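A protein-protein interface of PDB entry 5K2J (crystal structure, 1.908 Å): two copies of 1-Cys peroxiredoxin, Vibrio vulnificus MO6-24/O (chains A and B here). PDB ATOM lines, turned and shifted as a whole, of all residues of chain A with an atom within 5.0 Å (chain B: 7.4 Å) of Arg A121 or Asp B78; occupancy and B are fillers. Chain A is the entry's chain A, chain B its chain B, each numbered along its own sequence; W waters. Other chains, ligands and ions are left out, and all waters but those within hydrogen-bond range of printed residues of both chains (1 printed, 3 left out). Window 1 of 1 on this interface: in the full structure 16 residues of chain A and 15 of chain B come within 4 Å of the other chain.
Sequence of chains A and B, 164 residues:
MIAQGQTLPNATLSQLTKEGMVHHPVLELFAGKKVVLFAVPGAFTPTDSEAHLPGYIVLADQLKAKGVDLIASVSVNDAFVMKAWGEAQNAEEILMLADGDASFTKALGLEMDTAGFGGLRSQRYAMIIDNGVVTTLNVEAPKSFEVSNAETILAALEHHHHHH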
ATOM      1  N   PRO A  41      -2.434   6.688   0.809  1.00  0.00           N
ATOM      2  CA  PRO A  41      -2.733   6.878   2.238  1.00  0.00           C
ATOM      3  C   PRO A  41      -1.513   6.762   3.133  1.00  0.00           C
ATOM      4  O   PRO A  41      -1.484   7.387   4.199  1.00  0.00           O
ATOM      5  CB  PRO A  41      -3.757   5.773   2.535  1.00  0.00           C
ATOM      6  CG  PRO A  41      -4.358   5.448   1.198  1.00  0.00           C
ATOM      7  CD  PRO A  41      -3.239   5.607   0.216  1.00  0.00           C
ATOM      8  N   GLY A  42      -0.502   5.990   2.743  1.00  0.00           N
ATOM      9  CA  GLY A  42       0.696   5.919   3.554  1.00  0.00           C
ATOM     10  C   GLY A  42       1.825   5.134   2.924  1.00  0.00           C
ATOM     11  O   GLY A  42       1.588   4.135   2.240  1.00  0.00           O
ATOM     12  N   ALA A  43       3.061   5.578   3.141  1.00  0.00           N
ATOM     13  CA  ALA A  43       4.208   4.785   2.723  1.00  0.00           C
ATOM     14  C   ALA A  43       4.220   3.448   3.456  1.00  0.00           C
ATOM     15  O   ALA A  43       3.807   3.345   4.616  1.00  0.00           O
ATOM     16  CB  ALA A  43       5.511   5.543   2.989  1.00  0.00           C
ATOM     17  N   THR A  45       2.395   0.882   3.115  1.00  0.00           N
ATOM     18  CA  THR A  45       1.142   0.147   3.212  1.00  0.00           C
ATOM     19  C   THR A  45       0.962  -0.754   1.987  1.00  0.00           C
ATOM     20  O   THR A  45       1.544  -0.499   0.930  1.00  0.00           O
ATOM     21  CB  THR A  45      -0.030   1.114   3.357  1.00  0.00           C
ATOM     22  OG1 THR A  45      -0.110   1.959   2.205  1.00  0.00           O
ATOM     23  CG2 THR A  45       0.154   1.974   4.588  1.00  0.00           C
ATOM     24  N   VAL A  76       1.010  11.591   3.321  1.00  0.00           N
ATOM     25  CA  VAL A  76       1.138  12.186   4.645  1.00  0.00           C
ATOM     26  C   VAL A  76       2.109  11.330   5.446  1.00  0.00           C
ATOM     27  O   VAL A  76       1.706  10.517   6.286  1.00  0.00           O
ATOM     28  CB  VAL A  76      -0.228  12.334   5.334  1.00  0.00           C
ATOM     29  CG1 VAL A  76      -0.074  13.019   6.693  1.00  0.00           C
ATOM     30  CG2 VAL A  76      -1.164  13.138   4.439  1.00  0.00           C
ATOM     31  N   ASN A  77       3.394  11.474   5.127  1.00  0.00           N
ATOM     32  CA  ASN A  77       4.511  10.891   5.854  1.00  0.00           C
ATOM     33  C   ASN A  77       5.633  11.917   5.856  1.00  0.00           C
ATOM     34  O   ASN A  77       5.644  12.849   5.048  1.00  0.00           O
ATOM     35  CB  ASN A  77       5.034   9.596   5.213  1.00  0.00           C
ATOM     36  CG  ASN A  77       4.028   8.469   5.243  1.00  0.00           C
ATOM     37  OD1 ASN A  77       3.183   8.353   4.352  1.00  0.00           O
ATOM     38  ND2 ASN A  77       4.132   7.610   6.253  1.00  0.00           N
ATOM     39  N   THR A 105      -2.504  18.356   1.992  1.00  0.00           N
ATOM     40  CA  THR A 105      -3.680  17.524   1.762  1.00  0.00           C
ATOM     41  C   THR A 105      -4.946  18.184   2.301  1.00  0.00           C
ATOM     42  O   THR A 105      -5.993  18.154   1.646  1.00  0.00           O
ATOM     43  CB  THR A 105      -3.463  16.151   2.395  1.00  0.00           C
ATOM     44  OG1 THR A 105      -2.308  15.545   1.803  1.00  0.00           O
ATOM     45  CG2 THR A 105      -4.670  15.257   2.178  1.00  0.00           C
ATOM     46  N   LEU A 110      -8.765  16.930   0.729  1.00  0.00           N
ATOM     47  CA  LEU A 110      -8.719  15.513   0.391  1.00  0.00           C
ATOM     48  C   LEU A 110      -8.131  14.683   1.525  1.00  0.00           C
ATOM     49  O   LEU A 110      -7.588  13.600   1.298  1.00  0.00           O
ATOM     50  CB  LEU A 110      -7.931  15.300  -0.900  1.00  0.00           C
ATOM     51  CG  LEU A 110      -8.649  15.824  -2.144  1.00  0.00           C
ATOM     52  CD1 LEU A 110      -7.771  15.686  -3.371  1.00  0.00           C
ATOM     53  CD2 LEU A 110      -9.951  15.065  -2.328  1.00  0.00           C
ATOM     54  N   GLU A 111      -8.227  15.180   2.752  1.00  0.00           N
ATOM     55  CA  GLU A 111      -7.755  14.414   3.889  1.00  0.00           C
ATOM     56  C   GLU A 111      -8.830  13.430   4.338  1.00  0.00           C
ATOM     57  O   GLU A 111     -10.015  13.574   4.022  1.00  0.00           O
ATOM     58  CB  GLU A 111      -7.366  15.339   5.043  1.00  0.00           C
ATOM     59  CG  GLU A 111      -8.539  15.871   5.856  1.00  0.00           C
ATOM     60  CD  GLU A 111      -9.280  17.013   5.178  1.00  0.00           C
ATOM     61  OE1 GLU A 111      -8.976  17.327   4.006  1.00  0.00           O
ATOM     62  OE2 GLU A 111     -10.171  17.602   5.827  1.00  0.00           O
ATOM     63  N   MET A 112      -8.395  12.407   5.068  1.00  0.00           N
ATOM     64  CA  MET A 112      -9.300  11.436   5.664  1.00  0.00           C
ATOM     65  C   MET A 112      -8.723  11.001   7.001  1.00  0.00           C
ATOM     66  O   MET A 112      -7.505  11.008   7.200  1.00  0.00           O
ATOM     67  CB  MET A 112      -9.514  10.214   4.762  1.00  0.00           C
ATOM     68  CG  MET A 112      -8.285   9.340   4.610  1.00  0.00           C
ATOM     69  SD  MET A 112      -8.600   7.900   3.586  1.00  0.00           S
ATOM     70  CE  MET A 112     -10.148   7.341   4.287  1.00  0.00           C
ATOM     71  N   THR A 114      -7.985   8.176   9.472  1.00  0.00           N
ATOM     72  CA  THR A 114      -7.797   6.740   9.629  1.00  0.00           C
ATOM     73  C   THR A 114      -7.809   6.296  11.093  1.00  0.00           C
ATOM     74  O   THR A 114      -7.526   5.125  11.372  1.00  0.00           O
ATOM     75  CB  THR A 114      -6.484   6.302   8.977  1.00  0.00           C
ATOM     76  OG1 THR A 114      -5.397   7.011   9.580  1.00  0.00           O
ATOM     77  CG2 THR A 114      -6.493   6.604   7.489  1.00  0.00           C
ATOM     78  N   PHE A 117      -4.945   3.955  13.128  1.00  0.00           N
ATOM     79  CA  PHE A 117      -3.995   3.303  12.221  1.00  0.00           C
ATOM     80  C   PHE A 117      -2.590   3.961  12.070  1.00  0.00           C
ATOM     81  O   PHE A 117      -1.595   3.256  12.201  1.00  0.00           O
ATOM     82  CB  PHE A 117      -4.623   3.147  10.833  1.00  0.00           C
ATOM     83  CG  PHE A 117      -3.624   2.836   9.766  1.00  0.00           C
ATOM     84  CD1 PHE A 117      -3.017   1.593   9.713  1.00  0.00           C
ATOM     85  CD2 PHE A 117      -3.272   3.792   8.827  1.00  0.00           C
ATOM     86  CE1 PHE A 117      -2.083   1.306   8.740  1.00  0.00           C
ATOM     87  CE2 PHE A 117      -2.338   3.509   7.851  1.00  0.00           C
ATOM     88  CZ  PHE A 117      -1.743   2.263   7.809  1.00  0.00           C
ATOM     89  N   GLY A 118      -2.472   5.265  11.803  1.00  0.00           N
ATOM     90  CA  GLY A 118      -3.578   6.191  11.733  1.00  0.00           C
ATOM     91  C   GLY A 118      -3.281   7.670  11.595  1.00  0.00           C
ATOM     92  O   GLY A 118      -2.364   8.093  10.879  1.00  0.00           O
ATOM     93  N   GLY A 119      -4.089   8.462  12.293  1.00  0.00           N
ATOM     94  CA  GLY A 119      -4.082   9.894  12.143  1.00  0.00           C
ATOM     95  C   GLY A 119      -4.734  10.307  10.833  1.00  0.00           C
ATOM     96  O   GLY A 119      -5.329   9.510  10.102  1.00  0.00           O
ATOM     97  N   LEU A 120      -4.614  11.598  10.549  1.00  0.00           N
ATOM     98  CA  LEU A 120      -5.052  12.120   9.264  1.00  0.00           C
ATOM     99  C   LEU A 120      -4.095  11.671   8.169  1.00  0.00           C
ATOM    100  O   LEU A 120      -2.877  11.848   8.284  1.00  0.00           O
ATOM    101  CB  LEU A 120      -5.127  13.645   9.304  1.00  0.00           C
ATOM    102  CG  LEU A 120      -6.463  14.280   9.685  1.00  0.00           C
ATOM    103  CD1 LEU A 120      -6.957  13.765  11.029  1.00  0.00           C
ATOM    104  CD2 LEU A 120      -6.333  15.799   9.698  1.00  0.00           C
ATOM    105  N   ARG A 121      -4.642  11.070   7.119  1.00  0.00           N
ATOM    106  CA  ARG A 121      -3.881  10.679   5.940  1.00  0.00           C
ATOM    107  C   ARG A 121      -4.571  11.259   4.712  1.00  0.00           C
ATOM    108  O   ARG A 121      -5.635  11.880   4.805  1.00  0.00           O
ATOM    109  CB  ARG A 121      -3.751   9.154   5.836  1.00  0.00           C
ATOM    110  CG  ARG A 121      -3.002   8.505   7.001  1.00  0.00           C
ATOM    111  CD  ARG A 121      -1.578   9.041   7.101  1.00  0.00           C
ATOM    112  NE  ARG A 121      -0.809   8.414   8.174  1.00  0.00           N
ATOM    113  CZ  ARG A 121       0.007   7.380   8.001  1.00  0.00           C
ATOM    114  NH1 ARG A 121       0.161   6.851   6.795  1.00  0.00           N
ATOM    115  NH2 ARG A 121       0.673   6.877   9.031  1.00  0.00           N
ATOM    116  N   SER A 122      -3.961  11.068   3.551  1.00  0.00           N
ATOM    117  CA  SER A 122      -4.547  11.550   2.310  1.00  0.00           C
ATOM    118  C   SER A 122      -5.476  10.496   1.734  1.00  0.00           C
ATOM    119  O   SER A 122      -5.209   9.296   1.835  1.00  0.00           O
ATOM    120  CB  SER A 122      -3.464  11.894   1.289  1.00  0.00           C
ATOM    121  OG  SER A 122      -4.037  12.368   0.080  1.00  0.00           O
ATOM    122  N   GLN A 123      -6.575  10.949   1.135  1.00  0.00           N
ATOM    123  CA  GLN A 123      -7.329  10.069   0.259  1.00  0.00           C
ATOM    124  C   GLN A 123      -6.468   9.693  -0.940  1.00  0.00           C
ATOM    125  O   GLN A 123      -5.543  10.415  -1.325  1.00  0.00           O
ATOM    126  CB  GLN A 123      -8.615  10.739  -0.219  1.00  0.00           C
ATOM    127  CG  GLN A 123      -9.568  11.150   0.884  1.00  0.00           C
ATOM    128  CD  GLN A 123     -10.823  11.797   0.339  1.00  0.00           C
ATOM    129  OE1 GLN A 123     -11.440  11.285  -0.593  1.00  0.00           O
ATOM    130  NE2 GLN A 123     -11.202  12.935   0.911  1.00  0.00           N
ATOM    131  N   SER B  14      -0.614  -0.666  18.246  1.00  0.00           N
ATOM    132  CA  SER B  14      -0.826  -1.606  17.158  1.00  0.00           C
ATOM    133  C   SER B  14       0.482  -2.256  16.727  1.00  0.00           C
ATOM    134  O   SER B  14       1.558  -1.656  16.804  1.00  0.00           O
ATOM    135  CB  SER B  14      -1.478  -0.913  15.959  1.00  0.00           C
ATOM    136  OG  SER B  14      -2.792  -0.491  16.279  1.00  0.00           O
ATOM    137  N   MET B  21      -2.998  -7.730  11.745  1.00  0.00           N
ATOM    138  CA  MET B  21      -2.950  -6.537  12.578  1.00  0.00           C
ATOM    139  C   MET B  21      -3.580  -6.827  13.934  1.00  0.00           C
ATOM    140  O   MET B  21      -4.672  -7.397  14.013  1.00  0.00           O
ATOM    141  CB  MET B  21      -3.679  -5.385  11.890  1.00  0.00           C
ATOM    142  CG  MET B  21      -3.449  -4.034  12.529  1.00  0.00           C
ATOM    143  SD  MET B  21      -1.922  -3.259  11.968  1.00  0.00           S
ATOM    144  CE  MET B  21      -2.316  -1.542  12.312  1.00  0.00           C
ATOM    145  N   ALA B  43      10.173   6.656  13.037  1.00  0.00           N
ATOM    146  CA  ALA B  43      10.961   5.635  12.361  1.00  0.00           C
ATOM    147  C   ALA B  43      11.707   6.233  11.171  1.00  0.00           C
ATOM    148  O   ALA B  43      11.247   7.187  10.535  1.00  0.00           O
ATOM    149  CB  ALA B  43      10.060   4.490  11.894  1.00  0.00           C
ATOM    150  N   SER B  75       6.457   4.551  18.580  1.00  0.00           N
ATOM    151  CA  SER B  75       6.597   5.770  17.801  1.00  0.00           C
ATOM    152  C   SER B  75       5.236   6.148  17.246  1.00  0.00           C
ATOM    153  O   SER B  75       4.377   5.286  17.045  1.00  0.00           O
ATOM    154  CB  SER B  75       7.596   5.597  16.654  1.00  0.00           C
ATOM    155  OG  SER B  75       7.745   6.806  15.936  1.00  0.00           O
ATOM    156  N   VAL B  76       5.039   7.448  17.015  1.00  0.00           N
ATOM    157  CA  VAL B  76       3.846   7.914  16.318  1.00  0.00           C
ATOM    158  C   VAL B  76       4.064   7.641  14.837  1.00  0.00           C
ATOM    159  O   VAL B  76       4.455   8.529  14.069  1.00  0.00           O
ATOM    160  CB  VAL B  76       3.547   9.399  16.600  1.00  0.00           C
ATOM    161  CG1 VAL B  76       2.283   9.844  15.868  1.00  0.00           C
ATOM    162  CG2 VAL B  76       3.389   9.627  18.096  1.00  0.00           C
ATOM    163  N   ASN B  77       3.876   6.382  14.457  1.00  0.00           N
ATOM    164  CA  ASN B  77       3.919   5.908  13.084  1.00  0.00           C
ATOM    165  C   ASN B  77       2.885   4.799  12.965  1.00  0.00           C
ATOM    166  O   ASN B  77       2.448   4.234  13.970  1.00  0.00           O
ATOM    167  CB  ASN B  77       5.307   5.367  12.690  1.00  0.00           C
ATOM    168  CG  ASN B  77       6.342   6.463  12.504  1.00  0.00           C
ATOM    169  OD1 ASN B  77       7.160   6.719  13.391  1.00  0.00           O
ATOM    170  ND2 ASN B  77       6.323   7.103  11.339  1.00  0.00           N
ATOM    171  N   ASP B  78       2.491   4.485  11.735  1.00  0.00           N
ATOM    172  CA  ASP B  78       1.614   3.340  11.552  1.00  0.00           C
ATOM    173  C   ASP B  78       2.403   2.040  11.696  1.00  0.00           C
ATOM    174  O   ASP B  78       3.636   2.018  11.646  1.00  0.00           O
ATOM    175  CB  ASP B  78       0.930   3.389  10.188  1.00  0.00           C
ATOM    176  CG  ASP B  78       1.918   3.384   9.049  1.00  0.00           C
ATOM    177  OD1 ASP B  78       2.348   2.286   8.640  1.00  0.00           O
ATOM    178  OD2 ASP B  78       2.264   4.481   8.559  1.00  0.00           O
ATOM    179  N   ALA B  79       1.669   0.938  11.867  1.00  0.00           N
ATOM    180  CA  ALA B  79       2.309  -0.351  12.101  1.00  0.00           C
ATOM    181  C   ALA B  79       3.054  -0.877  10.882  1.00  0.00           C
ATOM    182  O   ALA B  79       3.979  -1.682  11.041  1.00  0.00           O
ATOM    183  CB  ALA B  79       1.272  -1.378  12.557  1.00  0.00           C
ATOM    184  N   PHE B  80       2.673  -0.462   9.670  1.00  0.00           N
ATOM    185  CA  PHE B  80       3.422  -0.901   8.496  1.00  0.00           C
ATOM    186  C   PHE B  80       4.804  -0.263   8.458  1.00  0.00           C
ATOM    187  O   PHE B  80       5.794  -0.931   8.141  1.00  0.00           O
ATOM    188  CB  PHE B  80       2.641  -0.590   7.218  1.00  0.00           C
ATOM    189  CG  PHE B  80       1.382  -1.395   7.072  1.00  0.00           C
ATOM    190  CD1 PHE B  80       1.431  -2.704   6.626  1.00  0.00           C
ATOM    191  CD2 PHE B  80       0.152  -0.845   7.384  1.00  0.00           C
ATOM    192  CE1 PHE B  80       0.276  -3.452   6.496  1.00  0.00           C
ATOM    193  CE2 PHE B  80      -1.007  -1.586   7.253  1.00  0.00           C
ATOM    194  CZ  PHE B  80      -0.944  -2.892   6.810  1.00  0.00           C
ATOM    195  N   VAL B  81       4.893   1.026   8.791  1.00  0.00           N
ATOM    196  CA  VAL B  81       6.192   1.688   8.863  1.00  0.00           C
ATOM    197  C   VAL B  81       7.041   1.090   9.982  1.00  0.00           C
ATOM    198  O   VAL B  81       8.241   0.846   9.803  1.00  0.00           O
ATOM    199  CB  VAL B  81       6.004   3.207   9.038  1.00  0.00           C
ATOM    200  CG1 VAL B  81       7.331   3.885   9.367  1.00  0.00           C
ATOM    201  CG2 VAL B  81       5.394   3.815   7.783  1.00  0.00           C
ATOM    202  N   MET B  82       6.436   0.835  11.149  1.00  0.00           N
ATOM    203  CA  MET B  82       7.197   0.283  12.268  1.00  0.00           C
ATOM    204  C   MET B  82       7.763  -1.091  11.935  1.00  0.00           C
ATOM    205  O   MET B  82       8.911  -1.397  12.279  1.00  0.00           O
ATOM    206  CB  MET B  82       6.326   0.209  13.524  1.00  0.00           C
ATOM    207  CG  MET B  82       5.994   1.569  14.123  1.00  0.00           C
ATOM    208  SD  MET B  82       7.467   2.502  14.599  1.00  0.00           S
ATOM    209  CE  MET B  82       8.001   1.631  16.073  1.00  0.00           C
ATOM    210  N   LYS B  83       6.978  -1.933  11.258  1.00  0.00           N
ATOM    211  CA  LYS B  83       7.464  -3.262  10.901  1.00  0.00           C
ATOM    212  C   LYS B  83       8.620  -3.182   9.911  1.00  0.00           C
ATOM    213  O   LYS B  83       9.635  -3.869  10.080  1.00  0.00           O
ATOM    214  CB  LYS B  83       6.322  -4.104  10.334  1.00  0.00           C
ATOM    215  CG  LYS B  83       6.767  -5.428   9.740  1.00  0.00           C
ATOM    216  CD  LYS B  83       5.589  -6.364   9.527  1.00  0.00           C
ATOM    217  CE  LYS B  83       5.553  -6.895   8.103  1.00  0.00           C
ATOM    218  NZ  LYS B  83       6.808  -7.608   7.738  1.00  0.00           N
ATOM    219  N   ALA B  84       8.490  -2.347   8.877  1.00  0.00           N
ATOM    220  CA  ALA B  84       9.574  -2.198   7.909  1.00  0.00           C
ATOM    221  C   ALA B  84      10.813  -1.581   8.541  1.00  0.00           C
ATOM    222  O   ALA B  84      11.938  -1.901   8.140  1.00  0.00           O
ATOM    223  CB  ALA B  84       9.108  -1.353   6.723  1.00  0.00           C
ATOM    224  N   LEU B  97       6.083  -1.168  18.321  1.00  0.00           N
ATOM    225  CA  LEU B  97       4.705  -0.787  18.591  1.00  0.00           C
ATOM    226  C   LEU B  97       4.389   0.542  17.920  1.00  0.00           C
ATOM    227  O   LEU B  97       5.214   1.462  17.925  1.00  0.00           O
ATOM    228  CB  LEU B  97       4.457  -0.690  20.100  1.00  0.00           C
ATOM    229  CG  LEU B  97       4.613  -2.016  20.846  1.00  0.00           C
ATOM    230  CD1 LEU B  97       4.521  -1.818  22.352  1.00  0.00           C
ATOM    231  CD2 LEU B  97       3.564  -3.007  20.366  1.00  0.00           C
ATOM    232  N   ALA B  98       3.188   0.638  17.353  1.00  0.00           N
ATOM    233  CA  ALA B  98       2.761   1.804  16.592  1.00  0.00           C
ATOM    234  C   ALA B  98       1.676   2.555  17.347  1.00  0.00           C
ATOM    235  O   ALA B  98       0.713   1.948  17.829  1.00  0.00           O
ATOM    236  CB  ALA B  98       2.245   1.392  15.213  1.00  0.00           C
ATOM    237  N   ASP B  99       1.833   3.872  17.442  1.00  0.00           N
ATOM    238  CA  ASP B  99       0.832   4.781  18.003  1.00  0.00           C
ATOM    239  C   ASP B  99       0.380   5.702  16.866  1.00  0.00           C
ATOM    240  O   ASP B  99       0.768   6.871  16.801  1.00  0.00           O
ATOM    241  CB  ASP B  99       1.424   5.561  19.186  1.00  0.00           C
ATOM    242  CG  ASP B  99       0.399   6.424  19.890  1.00  0.00           C
ATOM    243  OD1 ASP B  99      -0.804   6.092  19.847  1.00  0.00           O
ATOM    244  OD2 ASP B  99       0.807   7.438  20.494  1.00  0.00           O
ATOM    245  N   GLY B 100      -0.461   5.161  15.979  1.00  0.00           N
ATOM    246  CA  GLY B 100      -0.691   5.796  14.687  1.00  0.00           C
ATOM    247  C   GLY B 100      -1.272   7.194  14.779  1.00  0.00           C
ATOM    248  O   GLY B 100      -0.848   8.098  14.055  1.00  0.00           O
ATOM    249  N   ASP B 101      -2.267   7.388  15.643  1.00  0.00           N
ATOM    250  CA  ASP B 101      -2.908   8.687  15.799  1.00  0.00           C
ATOM    251  C   ASP B 101      -2.387   9.456  17.001  1.00  0.00           C
ATOM    252  O   ASP B 101      -2.980  10.474  17.375  1.00  0.00           O
ATOM    253  CB  ASP B 101      -4.425   8.528  15.904  1.00  0.00           C
ATOM    254  CG  ASP B 101      -4.850   7.758  17.139  1.00  0.00           C
ATOM    255  OD1 ASP B 101      -4.011   7.028  17.712  1.00  0.00           O
ATOM    256  OD2 ASP B 101      -6.031   7.881  17.532  1.00  0.00           O
HETATM  257  O   HOH W   1       1.052   7.962  11.740  1.00  0.00           O
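Val B81 touches Ala A43 (CG2 to O, 3.6 Å). CG2 of Thr A45 touches CD2 of Phe B80 (3.97 Å). O of Phe A117 touches CB of Asp B78, 3.2 Å away. CD2 of Phe B80 touches CE1 of Phe A117, at 3.4 Å. Gly B100 touches Phe A117. Gly A118 touches Gly B100 (N to CA, 3.4 Å). N of Gly A119 touches O of Gly B100, 3.7 Å away. CB of Asp B101 touches N of Gly A119 (3.6 Å).
Of the printed residues of chain B, Ala A43 touches Val B81 (3.6 Å). Glu A111 touches none of the printed residues of chain B. Printed residues of chain B within 4 Å of Phe A117: Asp B78, Phe B80 and Gly B100. Of chain B, only Asp B78 (2.9 Å) comes within 4 Å of Arg A121. Ala B43 touches none of the printed residues of chain A. Of chain A, only Phe A117 (3.2 Å) and Arg A121 (2.9 Å) come within 4 Å of Asp B78. The nearest residue of chain A that does not touch Asp B78 is Gly A118 (4.2 Å). The nearest printed residue of chain A that does not touch Asp B101 is Gly A118 (4.2 Å).
The guanidinium group (NH1) of Arg A121 lies within hydrogen-bond range of the backbone carbonyl oxygen (O) of Pro A41, 3.1 Å away. N of Ala A43 sits at hydrogen-bond distance from OD1 of Asn A77, at 3.0 Å. The backbone NH (N) of Met A112 sits at hydrogen-bond distance from the backbone carbonyl oxygen (O) of Arg A121 (2.8 Å). The side-chain hydroxyl (OG1) of Thr A114 sits close to the backbone carbonyl oxygen (O) of Gly A118 (3.5 Å). The side-chain hydroxyl of Thr A114 lies within hydrogen-bond range of the backbone carbonyl oxygen of Gly A119 (2.6 Å). The guanidinium group of Arg A121 sits at hydrogen-bond distance from the backbone carbonyl oxygen of Gly A118, at 3.1 Å.
Water W1 bridges NH2 of Arg A121 and O of Gly B100.
3 positions are printed for both chains. Of the 9 pairs that touch across the chains among the printed residues, none has its exchanged pair printed and touching as well.
Hydrophobic or aromatic side chains of chain A that line the printed part of chain B: Phe A117. Among the printed residues, Asp or Glu carboxylates within 4 Å of a Lys or Arg side-chain nitrogen of the other chain: Arg A121 with Asp B78 (2.9 Å).
The guanidinium group of Arg A121 lies within salt-bridge range of the side-chain carboxylate of Asp B78, 2.9 Å away.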
